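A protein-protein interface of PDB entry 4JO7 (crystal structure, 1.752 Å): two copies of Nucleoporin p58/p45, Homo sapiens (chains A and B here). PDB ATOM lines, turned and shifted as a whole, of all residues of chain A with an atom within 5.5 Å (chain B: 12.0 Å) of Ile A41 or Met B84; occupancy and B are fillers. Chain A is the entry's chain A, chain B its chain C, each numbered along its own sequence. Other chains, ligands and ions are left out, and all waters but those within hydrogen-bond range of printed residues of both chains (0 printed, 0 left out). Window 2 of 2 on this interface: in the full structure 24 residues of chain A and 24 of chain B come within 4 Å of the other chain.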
ATOM      1  N   THR A  34      15.246 -14.486 -16.748  1.00  0.00           N
ATOM      2  CA  THR A  34      14.089 -13.774 -16.217  1.00  0.00           C
ATOM      3  C   THR A  34      13.614 -14.294 -14.862  1.00  0.00           C
ATOM      4  O   THR A  34      14.147 -15.265 -14.323  1.00  0.00           O
ATOM      5  CB  THR A  34      12.903 -13.841 -17.199  1.00  0.00           C
ATOM      6  OG1 THR A  34      12.452 -15.195 -17.318  1.00  0.00           O
ATOM      7  CG2 THR A  34      13.313 -13.322 -18.569  1.00  0.00           C
ATOM      8  N   GLN A  35      12.599 -13.623 -14.328  1.00  0.00           N
ATOM      9  CA  GLN A  35      12.000 -13.952 -13.042  1.00  0.00           C
ATOM     10  C   GLN A  35      12.899 -13.879 -11.829  1.00  0.00           C
ATOM     11  O   GLN A  35      12.446 -14.220 -10.728  1.00  0.00           O
ATOM     12  CB  GLN A  35      11.378 -15.336 -13.093  1.00  0.00           C
ATOM     13  CG  GLN A  35      10.855 -15.722 -14.450  1.00  0.00           C
ATOM     14  CD  GLN A  35      10.539 -17.172 -14.547  1.00  0.00           C
ATOM     15  OE1 GLN A  35      11.102 -17.905 -15.360  1.00  0.00           O
ATOM     16  NE2 GLN A  35       9.612 -17.601 -13.716  1.00  0.00           N
ATOM     17  N   SER A  39       9.434 -11.086 -10.755  1.00  0.00           N
ATOM     18  CA  SER A  39       8.487 -11.018 -11.889  1.00  0.00           C
ATOM     19  C   SER A  39       8.063 -12.355 -12.487  1.00  0.00           C
ATOM     20  O   SER A  39       8.644 -13.382 -12.225  1.00  0.00           O
ATOM     21  CB  SER A  39       8.972  -9.987 -12.965  1.00  0.00           C
ATOM     22  OG  SER A  39       9.181 -10.530 -14.260  1.00  0.00           O
ATOM     23  N   HIS A  40       6.963 -12.318 -13.234  1.00  0.00           N
ATOM     24  CA  HIS A  40       6.323 -13.524 -13.724  1.00  0.00           C
ATOM     25  C   HIS A  40       6.188 -13.496 -15.215  1.00  0.00           C
ATOM     26  O   HIS A  40       5.068 -13.430 -15.766  1.00  0.00           O
ATOM     27  CB  HIS A  40       4.952 -13.693 -13.078  1.00  0.00           C
ATOM     28  CG  HIS A  40       5.001 -13.836 -11.575  1.00  0.00           C
ATOM     29  ND1 HIS A  40       4.472 -14.893 -10.931  1.00  0.00           N
ATOM     30  CD2 HIS A  40       5.541 -13.007 -10.594  1.00  0.00           C
ATOM     31  CE1 HIS A  40       4.663 -14.750  -9.606  1.00  0.00           C
ATOM     32  NE2 HIS A  40       5.317 -13.597  -9.400  1.00  0.00           N
ATOM     33  N   ILE A  41       7.330 -13.545 -15.885  1.00  0.00           N
ATOM     34  CA  ILE A  41       7.388 -13.548 -17.325  1.00  0.00           C
ATOM     35  C   ILE A  41       8.432 -14.551 -17.693  1.00  0.00           C
ATOM     36  O   ILE A  41       9.592 -14.400 -17.409  1.00  0.00           O
ATOM     37  CB  ILE A  41       7.720 -12.155 -17.899  1.00  0.00           C
ATOM     38  CG1 ILE A  41       6.514 -11.269 -17.777  1.00  0.00           C
ATOM     39  CG2 ILE A  41       8.230 -12.231 -19.331  1.00  0.00           C
ATOM     40  CD1 ILE A  41       5.236 -11.829 -18.293  1.00  0.00           C
ATOM     41  N   THR A  42       7.961 -15.587 -18.313  1.00  0.00           N
ATOM     42  CA  THR A  42       8.799 -16.674 -18.780  1.00  0.00           C
ATOM     43  C   THR A  42       9.286 -16.383 -20.189  1.00  0.00           C
ATOM     44  O   THR A  42       8.654 -15.618 -20.919  1.00  0.00           O
ATOM     45  CB  THR A  42       8.019 -17.996 -18.797  1.00  0.00           C
ATOM     46  OG1 THR A  42       6.969 -17.918 -19.768  1.00  0.00           O
ATOM     47  CG2 THR A  42       7.418 -18.282 -17.427  1.00  0.00           C
ATOM     48  N   PRO A  43      10.420 -16.984 -20.573  1.00  0.00           N
ATOM     49  CA  PRO A  43      10.882 -16.870 -21.959  1.00  0.00           C
ATOM     50  C   PRO A  43       9.789 -17.275 -22.938  1.00  0.00           C
ATOM     51  O   PRO A  43       9.732 -16.745 -24.047  1.00  0.00           O
ATOM     52  CB  PRO A  43      12.052 -17.861 -22.035  1.00  0.00           C
ATOM     53  CG  PRO A  43      12.231 -18.430 -20.641  1.00  0.00           C
ATOM     54  CD  PRO A  43      11.425 -17.609 -19.700  1.00  0.00           C
ATOM     55  N   ASP A  45       6.562 -16.806 -22.582  1.00  0.00           N
ATOM     56  CA  ASP A  45       5.632 -15.691 -22.704  1.00  0.00           C
ATOM     57  C   ASP A  45       6.128 -14.717 -23.762  1.00  0.00           C
ATOM     58  O   ASP A  45       5.359 -14.235 -24.600  1.00  0.00           O
ATOM     59  CB  ASP A  45       5.488 -14.949 -21.375  1.00  0.00           C
ATOM     60  CG  ASP A  45       4.612 -15.683 -20.383  1.00  0.00           C
ATOM     61  OD1 ASP A  45       3.689 -16.403 -20.817  1.00  0.00           O
ATOM     62  OD2 ASP A  45       4.841 -15.526 -19.164  1.00  0.00           O
ATOM     63  N   LEU A  46       7.418 -14.407 -23.694  1.00  0.00           N
ATOM     64  CA  LEU A  46       8.033 -13.482 -24.635  1.00  0.00           C
ATOM     65  C   LEU A  46       7.999 -14.067 -26.035  1.00  0.00           C
ATOM     66  O   LEU A  46       7.708 -13.364 -27.004  1.00  0.00           O
ATOM     67  CB  LEU A  46       9.473 -13.189 -24.223  1.00  0.00           C
ATOM     68  CG  LEU A  46       9.642 -12.283 -23.001  1.00  0.00           C
ATOM     69  CD1 LEU A  46      11.053 -12.390 -22.470  1.00  0.00           C
ATOM     70  CD2 LEU A  46       9.332 -10.840 -23.346  1.00  0.00           C
ATOM     71  N   ALA A  49       4.566 -13.783 -27.606  1.00  0.00           N
ATOM     72  CA  ALA A  49       4.350 -12.393 -28.003  1.00  0.00           C
ATOM     73  C   ALA A  49       5.105 -12.053 -29.289  1.00  0.00           C
ATOM     74  O   ALA A  49       4.555 -11.412 -30.192  1.00  0.00           O
ATOM     75  CB  ALA A  49       4.758 -11.452 -26.885  1.00  0.00           C
ATOM     76  N   LYS B  75       1.969  -1.533 -32.992  1.00  0.00           N
ATOM     77  CA  LYS B  75       2.381  -0.620 -31.923  1.00  0.00           C
ATOM     78  C   LYS B  75       2.028  -1.186 -30.546  1.00  0.00           C
ATOM     79  O   LYS B  75       2.844  -1.144 -29.626  1.00  0.00           O
ATOM     80  CB  LYS B  75       1.726   0.744 -32.092  1.00  0.00           C
ATOM     81  CG  LYS B  75       2.204   1.531 -33.291  1.00  0.00           C
ATOM     82  CD  LYS B  75       1.407   2.820 -33.425  1.00  0.00           C
ATOM     83  CE  LYS B  75       1.910   3.703 -34.554  1.00  0.00           C
ATOM     84  NZ  LYS B  75       1.193   5.003 -34.579  1.00  0.00           N
ATOM     85  N   GLU B  76       0.815  -1.720 -30.415  1.00  0.00           N
ATOM     86  CA  GLU B  76       0.367  -2.312 -29.155  1.00  0.00           C
ATOM     87  C   GLU B  76       1.186  -3.549 -28.796  1.00  0.00           C
ATOM     88  O   GLU B  76       1.521  -3.766 -27.633  1.00  0.00           O
ATOM     89  CB  GLU B  76      -1.118  -2.672 -29.229  1.00  0.00           C
ATOM     90  CG  GLU B  76      -2.028  -1.459 -29.341  1.00  0.00           C
ATOM     91  CD  GLU B  76      -3.461  -1.815 -29.701  1.00  0.00           C
ATOM     92  OE1 GLU B  76      -3.756  -3.013 -29.890  1.00  0.00           O
ATOM     93  OE2 GLU B  76      -4.291  -0.888 -29.800  1.00  0.00           O
ATOM     94  N   GLN B  77       1.512  -4.356 -29.798  1.00  0.00           N
ATOM     95  CA  GLN B  77       2.329  -5.537 -29.570  1.00  0.00           C
ATOM     96  C   GLN B  77       3.747  -5.154 -29.120  1.00  0.00           C
ATOM     97  O   GLN B  77       4.325  -5.795 -28.239  1.00  0.00           O
ATOM     98  CB  GLN B  77       2.359  -6.410 -30.824  1.00  0.00           C
ATOM     99  CG  GLN B  77       1.029  -7.110 -31.090  1.00  0.00           C
ATOM    100  CD  GLN B  77       0.982  -7.832 -32.431  1.00  0.00           C
ATOM    101  OE1 GLN B  77       1.708  -7.490 -33.371  1.00  0.00           O
ATOM    102  NE2 GLN B  77       0.123  -8.840 -32.523  1.00  0.00           N
ATOM    103  N   TYR B  78       4.296  -4.103 -29.723  1.00  0.00           N
ATOM    104  CA  TYR B  78       5.628  -3.629 -29.367  1.00  0.00           C
ATOM    105  C   TYR B  78       5.633  -3.174 -27.915  1.00  0.00           C
ATOM    106  O   TYR B  78       6.532  -3.527 -27.143  1.00  0.00           O
ATOM    107  CB  TYR B  78       6.042  -2.452 -30.252  1.00  0.00           C
ATOM    108  CG  TYR B  78       6.668  -2.805 -31.580  1.00  0.00           C
ATOM    109  CD1 TYR B  78       6.578  -4.084 -32.121  1.00  0.00           C
ATOM    110  CD2 TYR B  78       7.376  -1.846 -32.289  1.00  0.00           C
ATOM    111  CE1 TYR B  78       7.167  -4.386 -33.347  1.00  0.00           C
ATOM    112  CE2 TYR B  78       7.963  -2.136 -33.504  1.00  0.00           C
ATOM    113  CZ  TYR B  78       7.861  -3.404 -34.029  1.00  0.00           C
ATOM    114  OH  TYR B  78       8.466  -3.668 -35.244  1.00  0.00           O
ATOM    115  N   LEU B  79       4.626  -2.387 -27.544  1.00  0.00           N
ATOM    116  CA  LEU B  79       4.521  -1.878 -26.177  1.00  0.00           C
ATOM    117  C   LEU B  79       4.353  -3.031 -25.193  1.00  0.00           C
ATOM    118  O   LEU B  79       4.951  -3.036 -24.117  1.00  0.00           O
ATOM    119  CB  LEU B  79       3.363  -0.885 -26.052  1.00  0.00           C
ATOM    120  CG  LEU B  79       3.563   0.445 -26.782  1.00  0.00           C
ATOM    121  CD1 LEU B  79       2.329   1.328 -26.642  1.00  0.00           C
ATOM    122  CD2 LEU B  79       4.803   1.172 -26.272  1.00  0.00           C
ATOM    123  N   GLY B  80       3.558  -4.021 -25.577  1.00  0.00           N
ATOM    124  CA  GLY B  80       3.350  -5.199 -24.753  1.00  0.00           C
ATOM    125  C   GLY B  80       4.625  -5.988 -24.524  1.00  0.00           C
ATOM    126  O   GLY B  80       4.918  -6.395 -23.396  1.00  0.00           O
ATOM    127  N   TYR B  81       5.388  -6.210 -25.591  1.00  0.00           N
ATOM    128  CA  TYR B  81       6.637  -6.953 -25.490  1.00  0.00           C
ATOM    129  C   TYR B  81       7.670  -6.180 -24.674  1.00  0.00           C
ATOM    130  O   TYR B  81       8.397  -6.756 -23.854  1.00  0.00           O
ATOM    131  CB  TYR B  81       7.196  -7.238 -26.878  1.00  0.00           C
ATOM    132  CG  TYR B  81       8.399  -8.147 -26.861  1.00  0.00           C
ATOM    133  CD1 TYR B  81       8.251  -9.526 -26.935  1.00  0.00           C
ATOM    134  CD2 TYR B  81       9.684  -7.629 -26.761  1.00  0.00           C
ATOM    135  CE1 TYR B  81       9.347 -10.363 -26.920  1.00  0.00           C
ATOM    136  CE2 TYR B  81      10.794  -8.460 -26.751  1.00  0.00           C
ATOM    137  CZ  TYR B  81      10.619  -9.824 -26.828  1.00  0.00           C
ATOM    138  OH  TYR B  81      11.716 -10.653 -26.816  1.00  0.00           O
ATOM    139  N   ARG B  82       7.734  -4.874 -24.914  1.00  0.00           N
ATOM    140  CA  ARG B  82       8.631  -3.990 -24.173  1.00  0.00           C
ATOM    141  C   ARG B  82       8.361  -4.087 -22.672  1.00  0.00           C
ATOM    142  O   ARG B  82       9.286  -4.244 -21.864  1.00  0.00           O
ATOM    143  CB  ARG B  82       8.435  -2.546 -24.641  1.00  0.00           C
ATOM    144  CG  ARG B  82       9.424  -1.556 -24.056  1.00  0.00           C
ATOM    145  CD  ARG B  82       8.997  -0.117 -24.319  1.00  0.00           C
ATOM    146  NE  ARG B  82       8.931   0.192 -25.745  1.00  0.00           N
ATOM    147  CZ  ARG B  82       8.572   1.370 -26.240  1.00  0.00           C
ATOM    148  NH1 ARG B  82       8.233   2.368 -25.431  1.00  0.00           N
ATOM    149  NH2 ARG B  82       8.546   1.549 -27.549  1.00  0.00           N
ATOM    150  N   LYS B  83       7.089  -3.980 -22.302  1.00  0.00           N
ATOM    151  CA  LYS B  83       6.691  -4.066 -20.902  1.00  0.00           C
ATOM    152  C   LYS B  83       7.136  -5.390 -20.287  1.00  0.00           C
ATOM    153  O   LYS B  83       7.694  -5.412 -19.187  1.00  0.00           O
ATOM    154  CB  LYS B  83       5.178  -3.877 -20.750  1.00  0.00           C
ATOM    155  CG  LYS B  83       4.718  -2.440 -20.906  1.00  0.00           C
ATOM    156  CD  LYS B  83       3.290  -2.254 -20.414  1.00  0.00           C
ATOM    157  CE  LYS B  83       2.826  -0.814 -20.576  1.00  0.00           C
ATOM    158  NZ  LYS B  83       2.530  -0.470 -21.996  1.00  0.00           N
ATOM    159  N   MET B  84       6.906  -6.491 -20.997  1.00  0.00           N
ATOM    160  CA  MET B  84       7.330  -7.798 -20.519  1.00  0.00           C
ATOM    161  C   MET B  84       8.843  -7.868 -20.348  1.00  0.00           C
ATOM    162  O   MET B  84       9.341  -8.349 -19.333  1.00  0.00           O
ATOM    163  CB  MET B  84       6.887  -8.896 -21.486  1.00  0.00           C
ATOM    164  CG  MET B  84       5.412  -9.210 -21.437  1.00  0.00           C
ATOM    165  SD  MET B  84       4.991 -10.613 -22.727  1.00  0.00           S
ATOM    166  CE  MET B  84       6.303 -11.916 -22.165  1.00  0.00           C
ATOM    167  N   PHE B  85       9.581  -7.395 -21.347  1.00  0.00           N
ATOM    168  CA  PHE B  85      11.031  -7.515 -21.327  1.00  0.00           C
ATOM    169  C   PHE B  85      11.613  -6.692 -20.174  1.00  0.00           C
ATOM    170  O   PHE B  85      12.563  -7.111 -19.508  1.00  0.00           O
ATOM    171  CB  PHE B  85      11.621  -7.054 -22.660  1.00  0.00           C
ATOM    172  CG  PHE B  85      13.030  -7.522 -22.897  1.00  0.00           C
ATOM    173  CD1 PHE B  85      14.097  -6.881 -22.293  1.00  0.00           C
ATOM    174  CD2 PHE B  85      13.286  -8.602 -23.728  1.00  0.00           C
ATOM    175  CE1 PHE B  85      15.394  -7.305 -22.512  1.00  0.00           C
ATOM    176  CE2 PHE B  85      14.572  -9.028 -23.953  1.00  0.00           C
ATOM    177  CZ  PHE B  85      15.633  -8.377 -23.340  1.00  0.00           C
ATOM    178  N   LEU B  86      11.034  -5.523 -19.941  1.00  0.00           N
ATOM    179  CA  LEU B  86      11.556  -4.603 -18.935  1.00  0.00           C
ATOM    180  C   LEU B  86      11.028  -4.890 -17.534  1.00  0.00           C
ATOM    181  O   LEU B  86      11.304  -4.139 -16.604  1.00  0.00           O
ATOM    182  CB  LEU B  86      11.246  -3.159 -19.329  1.00  0.00           C
ATOM    183  CG  LEU B  86      11.885  -2.685 -20.635  1.00  0.00           C
ATOM    184  CD1 LEU B  86      11.470  -1.257 -20.931  1.00  0.00           C
ATOM    185  CD2 LEU B  86      13.406  -2.802 -20.576  1.00  0.00           C
ATOM    186  N   GLY B  87      10.278  -5.980 -17.383  1.00  0.00           N
ATOM    187  CA  GLY B  87       9.771  -6.384 -16.084  1.00  0.00           C
ATOM    188  C   GLY B  87       8.592  -5.548 -15.624  1.00  0.00           C
ATOM    189  O   GLY B  87       8.332  -5.437 -14.428  1.00  0.00           O
ATOM    190  N   ASP B  88       7.885  -4.964 -16.587  1.00  0.00           N
ATOM    191  CA  ASP B  88       6.720  -4.120 -16.326  1.00  0.00           C
ATOM    192  C   ASP B  88       7.039  -2.911 -15.458  1.00  0.00           C
ATOM    193  O   ASP B  88       6.210  -2.007 -15.322  1.00  0.00           O
ATOM    194  CB  ASP B  88       5.589  -4.934 -15.694  1.00  0.00           C
ATOM    195  CG  ASP B  88       4.833  -5.760 -16.709  1.00  0.00           C
ATOM    196  OD1 ASP B  88       3.888  -5.221 -17.323  1.00  0.00           O
ATOM    197  OD2 ASP B  88       5.182  -6.943 -16.899  1.00  0.00           O
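O of Ile A41 sits at hydrogen-bond distance from OG1 of Thr A34, at 3.0 Å.
The backbone NH of Asp A45 is in hydrogen-bond range of the side-chain hydroxyl of Thr A42, at 3.1 Å.
CE of Met B84 touches CG2 of Ile A41 (3.4 Å).
C of Asp A45 touches CE of Met B84 (3.2 Å).
Leu A46 touches Tyr B81 (O to CE1, 3.4 Å).
CE of Met B84 touches N of Leu A46 (3.1 Å).
N of Phe B85 touches CD2 of Leu A46 (3.99 Å).
Ala A49 touches Tyr B81 (CB to CD1, 3.99 Å).
Ile A41 touches just one residue of chain B: Met B84.
Met B84 touches just these residues of chain A: Ile A41 (3.4 Å), Asp A45 (3.2 Å) and Leu A46 (3.1 Å).
No residue of chain B comes within 4 Å of Thr A34.
No residue of chain B comes within 4 Å of Gln A35.
No residue of chain B comes within 4 Å of Ser A39.
No residue of chain B comes within 4 Å of His A40.
No residue of chain B comes within 4 Å of Thr A42.
No residue of chain B comes within 4 Å of Pro A43.
Of the printed residues of chain A, Phe B85 touches Leu A46 (3.99 Å).
Printed residues of chain A within 4 Å of Tyr B81: Leu A46 (3.4 Å) and Ala A49 (3.99 Å).
The nearest residue of chain B that does not touch Ile A41 is Asp B88 (4.6 Å).
The nearest residue of chain A that does not touch Met B84 is Ala A49 (4.2 Å).
Hydrophobic or aromatic side chains of chain B within 4 Å of the printed part of chain A: Tyr B81 and Met B84.
Among the printed residues, 6 pairs touch across the chains.
No position is printed for both chains.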
